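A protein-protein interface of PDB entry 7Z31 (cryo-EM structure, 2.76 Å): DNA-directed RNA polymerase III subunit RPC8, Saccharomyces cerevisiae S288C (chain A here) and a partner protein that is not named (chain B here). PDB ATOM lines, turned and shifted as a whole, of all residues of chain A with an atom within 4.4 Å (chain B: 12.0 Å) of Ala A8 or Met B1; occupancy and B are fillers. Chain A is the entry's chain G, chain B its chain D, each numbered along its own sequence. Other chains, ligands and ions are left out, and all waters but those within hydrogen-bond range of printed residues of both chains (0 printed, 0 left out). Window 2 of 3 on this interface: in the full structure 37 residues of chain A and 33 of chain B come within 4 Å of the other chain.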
ATOM      1  N   ILE A   7      20.231  -9.259   2.576  1.00  0.00           N
ATOM      2  CA  ILE A   7      20.433  -8.211   3.565  1.00  0.00           C
ATOM      3  C   ILE A   7      19.076  -7.701   4.029  1.00  0.00           C
ATOM      4  O   ILE A   7      18.082  -7.771   3.302  1.00  0.00           O
ATOM      5  CB  ILE A   7      21.288  -7.058   2.998  1.00  0.00           C
ATOM      6  CG1 ILE A   7      22.519  -7.614   2.288  1.00  0.00           C
ATOM      7  CG2 ILE A   7      21.720  -6.105   4.094  1.00  0.00           C
ATOM      8  CD1 ILE A   7      23.453  -6.554   1.776  1.00  0.00           C
ATOM      9  N   ALA A   8      19.040  -7.200   5.259  1.00  0.00           N
ATOM     10  CA  ALA A   8      17.859  -6.578   5.838  1.00  0.00           C
ATOM     11  C   ALA A   8      18.183  -5.125   6.128  1.00  0.00           C
ATOM     12  O   ALA A   8      19.208  -4.829   6.750  1.00  0.00           O
ATOM     13  CB  ALA A   8      17.428  -7.285   7.122  1.00  0.00           C
ATOM     14  N   ASP A   9      17.319  -4.219   5.681  1.00  0.00           N
ATOM     15  CA  ASP A   9      17.607  -2.809   5.850  1.00  0.00           C
ATOM     16  C   ASP A   9      16.315  -2.034   6.041  1.00  0.00           C
ATOM     17  O   ASP A   9      15.220  -2.521   5.751  1.00  0.00           O
ATOM     18  CB  ASP A   9      18.390  -2.248   4.662  1.00  0.00           C
ATOM     19  CG  ASP A   9      19.252  -1.066   5.047  1.00  0.00           C
ATOM     20  OD1 ASP A   9      19.427  -0.823   6.260  1.00  0.00           O
ATOM     21  OD2 ASP A   9      19.754  -0.375   4.138  1.00  0.00           O
ATOM     22  N   LYS A  33      22.465   3.628  -1.287  1.00  0.00           N
ATOM     23  CA  LYS A  33      23.224   3.194  -0.121  1.00  0.00           C
ATOM     24  C   LYS A  33      24.318   2.181  -0.445  1.00  0.00           C
ATOM     25  O   LYS A  33      25.301   2.103   0.297  1.00  0.00           O
ATOM     26  CB  LYS A  33      22.280   2.607   0.927  1.00  0.00           C
ATOM     27  CG  LYS A  33      22.881   2.506   2.320  1.00  0.00           C
ATOM     28  CD  LYS A  33      21.904   1.870   3.289  1.00  0.00           C
ATOM     29  CE  LYS A  33      22.495   1.749   4.682  1.00  0.00           C
ATOM     30  NZ  LYS A  33      21.588   1.046   5.630  1.00  0.00           N
ATOM     31  N   ILE A  39      30.221  -3.631   1.838  1.00  0.00           N
ATOM     32  CA  ILE A  39      29.693  -3.954   3.168  1.00  0.00           C
ATOM     33  C   ILE A  39      30.853  -4.330   4.081  1.00  0.00           C
ATOM     34  O   ILE A  39      31.826  -4.944   3.609  1.00  0.00           O
ATOM     35  CB  ILE A  39      28.669  -5.088   3.073  1.00  0.00           C
ATOM     36  CG1 ILE A  39      27.450  -4.645   2.263  1.00  0.00           C
ATOM     37  CG2 ILE A  39      28.216  -5.529   4.450  1.00  0.00           C
ATOM     38  CD1 ILE A  39      27.519  -5.002   0.809  1.00  0.00           C
ATOM     39  N   PRO A  40      30.832  -3.954   5.358  1.00  0.00           N
ATOM     40  CA  PRO A  40      31.857  -4.453   6.279  1.00  0.00           C
ATOM     41  C   PRO A  40      31.877  -5.974   6.304  1.00  0.00           C
ATOM     42  O   PRO A  40      30.834  -6.625   6.399  1.00  0.00           O
ATOM     43  CB  PRO A  40      31.431  -3.868   7.629  1.00  0.00           C
ATOM     44  CG  PRO A  40      30.694  -2.639   7.284  1.00  0.00           C
ATOM     45  CD  PRO A  40      30.000  -2.908   5.976  1.00  0.00           C
ATOM     46  N   VAL A  70      13.062  -3.721   4.710  1.00  0.00           N
ATOM     47  CA  VAL A  70      13.178  -4.393   3.425  1.00  0.00           C
ATOM     48  C   VAL A  70      14.254  -5.467   3.502  1.00  0.00           C
ATOM     49  O   VAL A  70      15.278  -5.294   4.171  1.00  0.00           O
ATOM     50  CB  VAL A  70      13.468  -3.387   2.292  1.00  0.00           C
ATOM     51  CG1 VAL A  70      14.848  -2.786   2.445  1.00  0.00           C
ATOM     52  CG2 VAL A  70      13.306  -4.049   0.943  1.00  0.00           C
ATOM     53  N   THR A  71      13.998  -6.596   2.848  1.00  0.00           N
ATOM     54  CA  THR A  71      14.972  -7.668   2.689  1.00  0.00           C
ATOM     55  C   THR A  71      15.173  -7.897   1.201  1.00  0.00           C
ATOM     56  O   THR A  71      14.202  -8.033   0.453  1.00  0.00           O
ATOM     57  CB  THR A  71      14.511  -8.952   3.378  1.00  0.00           C
ATOM     58  OG1 THR A  71      14.533  -8.764   4.796  1.00  0.00           O
ATOM     59  CG2 THR A  71      15.421 -10.114   3.015  1.00  0.00           C
ATOM     60  N   MET B   1      20.644  -3.252   9.282  1.00  0.00           N
ATOM     61  CA  MET B   1      21.730  -3.354   8.320  1.00  0.00           C
ATOM     62  C   MET B   1      22.366  -4.738   8.397  1.00  0.00           C
ATOM     63  O   MET B   1      23.354  -5.021   7.721  1.00  0.00           O
ATOM     64  CB  MET B   1      22.765  -2.255   8.580  1.00  0.00           C
ATOM     65  CG  MET B   1      23.763  -2.024   7.458  1.00  0.00           C
ATOM     66  SD  MET B   1      25.393  -2.677   7.873  1.00  0.00           S
ATOM     67  CE  MET B   1      26.186  -2.642   6.271  1.00  0.00           C
ATOM     68  N   LYS B   2      21.791  -5.617   9.213  1.00  0.00           N
ATOM     69  CA  LYS B   2      22.416  -6.910   9.441  1.00  0.00           C
ATOM     70  C   LYS B   2      22.280  -7.805   8.215  1.00  0.00           C
ATOM     71  O   LYS B   2      21.212  -7.901   7.603  1.00  0.00           O
ATOM     72  CB  LYS B   2      21.823  -7.582  10.682  1.00  0.00           C
ATOM     73  CG  LYS B   2      20.379  -8.049  10.582  1.00  0.00           C
ATOM     74  CD  LYS B   2      19.885  -8.488  11.957  1.00  0.00           C
ATOM     75  CE  LYS B   2      18.663  -9.391  11.866  1.00  0.00           C
ATOM     76  NZ  LYS B   2      18.995 -10.731  11.313  1.00  0.00           N
ATOM     77  N   VAL B   3      23.383  -8.451   7.847  1.00  0.00           N
ATOM     78  CA  VAL B   3      23.395  -9.365   6.712  1.00  0.00           C
ATOM     79  C   VAL B   3      22.779 -10.681   7.160  1.00  0.00           C
ATOM     80  O   VAL B   3      23.319 -11.361   8.039  1.00  0.00           O
ATOM     81  CB  VAL B   3      24.821  -9.571   6.184  1.00  0.00           C
ATOM     82  CG1 VAL B   3      24.789 -10.201   4.809  1.00  0.00           C
ATOM     83  CG2 VAL B   3      25.567  -8.251   6.155  1.00  0.00           C
ATOM     84  N   LEU B   4      21.636 -11.037   6.568  1.00  0.00           N
ATOM     85  CA  LEU B   4      20.903 -12.212   7.031  1.00  0.00           C
ATOM     86  C   LEU B   4      21.724 -13.479   6.842  1.00  0.00           C
ATOM     87  O   LEU B   4      21.744 -14.356   7.715  1.00  0.00           O
ATOM     88  CB  LEU B   4      19.570 -12.318   6.298  1.00  0.00           C
ATOM     89  CG  LEU B   4      18.662 -11.107   6.483  1.00  0.00           C
ATOM     90  CD1 LEU B   4      17.267 -11.420   5.983  1.00  0.00           C
ATOM     91  CD2 LEU B   4      18.643 -10.709   7.940  1.00  0.00           C
ATOM     92  N   GLU B   5      22.402 -13.591   5.705  1.00  0.00           N
ATOM     93  CA  GLU B   5      23.364 -14.655   5.477  1.00  0.00           C
ATOM     94  C   GLU B   5      24.417 -14.122   4.518  1.00  0.00           C
ATOM     95  O   GLU B   5      24.175 -13.170   3.774  1.00  0.00           O
ATOM     96  CB  GLU B   5      22.686 -15.921   4.941  1.00  0.00           C
ATOM     97  CG  GLU B   5      21.744 -15.684   3.784  1.00  0.00           C
ATOM     98  CD  GLU B   5      22.481 -15.435   2.492  1.00  0.00           C
ATOM     99  OE1 GLU B   5      23.635 -15.891   2.381  1.00  0.00           O
ATOM    100  OE2 GLU B   5      21.917 -14.778   1.596  1.00  0.00           O
ATOM    101  N   GLU B   6      25.583 -14.760   4.532  1.00  0.00           N
ATOM    102  CA  GLU B   6      26.742 -14.265   3.800  1.00  0.00           C
ATOM    103  C   GLU B   6      26.780 -14.700   2.342  1.00  0.00           C
ATOM    104  O   GLU B   6      27.157 -13.904   1.476  1.00  0.00           O
ATOM    105  CB  GLU B   6      28.028 -14.715   4.499  1.00  0.00           C
ATOM    106  CG  GLU B   6      29.304 -14.248   3.822  1.00  0.00           C
ATOM    107  CD  GLU B   6      29.364 -12.745   3.651  1.00  0.00           C
ATOM    108  OE1 GLU B   6      28.708 -12.022   4.432  1.00  0.00           O
ATOM    109  OE2 GLU B   6      30.072 -12.286   2.732  1.00  0.00           O
ATOM    110  N   ARG B   7      26.400 -15.940   2.043  1.00  0.00           N
ATOM    111  CA  ARG B   7      26.515 -16.503   0.702  1.00  0.00           C
ATOM    112  C   ARG B   7      25.168 -17.084   0.295  1.00  0.00           C
ATOM    113  O   ARG B   7      24.694 -18.047   0.906  1.00  0.00           O
ATOM    114  CB  ARG B   7      27.602 -17.574   0.654  1.00  0.00           C
ATOM    115  CG  ARG B   7      27.735 -18.278  -0.683  1.00  0.00           C
ATOM    116  CD  ARG B   7      28.596 -19.530  -0.582  1.00  0.00           C
ATOM    117  NE  ARG B   7      29.889 -19.277   0.045  1.00  0.00           N
ATOM    118  CZ  ARG B   7      30.177 -19.552   1.308  1.00  0.00           C
ATOM    119  NH1 ARG B   7      29.280 -20.086   2.122  1.00  0.00           N
ATOM    120  NH2 ARG B   7      31.396 -19.283   1.769  1.00  0.00           N
ATOM    121  N   ASN B   8      24.549 -16.488  -0.715  1.00  0.00           N
ATOM    122  CA  ASN B   8      23.307 -16.982  -1.279  1.00  0.00           C
ATOM    123  C   ASN B   8      23.616 -17.728  -2.576  1.00  0.00           C
ATOM    124  O   ASN B   8      24.777 -17.997  -2.899  1.00  0.00           O
ATOM    125  CB  ASN B   8      22.316 -15.833  -1.485  1.00  0.00           C
ATOM    126  CG  ASN B   8      20.924 -16.170  -0.975  1.00  0.00           C
ATOM    127  OD1 ASN B   8      20.770 -16.796   0.074  1.00  0.00           O
ATOM    128  ND2 ASN B   8      19.904 -15.770  -1.725  1.00  0.00           N
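Ile A7 touches Lys B2. CB of Ala A8 touches CD2 of Leu B4, 3.7 Å away. OD1 of Asp A9 touches CA of Met B1 (3.99 Å). Met B1 touches Ile A39 (CE to CG2, 3.97 Å). Pro A40 touches Met B1 (CD to CE, 3.8 Å). Thr A71 touches Leu B4 (CG2 to CD1, 3.7 Å).
The backbone NH (N) of Ala A8 is in hydrogen-bond range of the backbone carbonyl oxygen (O) of Lys B2 (3.3 Å). N of Met B1 sits at hydrogen-bond distance from O of Ala A8 (3.3 Å).
Of the 8 printed residues of chain B, 3 touch a printed residue of chain A. Printed residues of chain B that touch a printed residue of chain A: Met B1, Lys B2 and Leu B4.
Ile A7 touches just one residue of chain B: Lys B2 (3.97 Å). Of the printed residues of chain B, Asp A9 touches Met B1. Ile A39 touches one residue of chain B. Pro A40 touches just one residue of chain B: Met B1 (3.8 Å). No residue of chain B comes within 4 Å of Val A70. Of the printed residues of chain B, Thr A71 touches Leu B4. Printed residues of chain A within 4 Å of Met B1: Ala A8 (3.3 Å), Asp A9 (3.99 Å), Ile A39 (3.97 Å) and Pro A40 (3.8 Å). Printed residues of chain A within 4 Å of Leu B4: Ala A8 (3.7 Å) and Thr A71 (3.7 Å). The nearest residue of chain B that does not touch Ala A8 is Val B3 (5.1 Å). The nearest printed residue of chain B that does not touch Asp A9 is Lys B2 (5.7 Å).
The side-chain amino group (NZ) of Lys A33 lies within salt-bridge range of the side-chain carboxylate (OD2) of Asp A9, 2.8 Å away. N of Val A70 lies within hydrogen-bond range of O of Asp A9.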
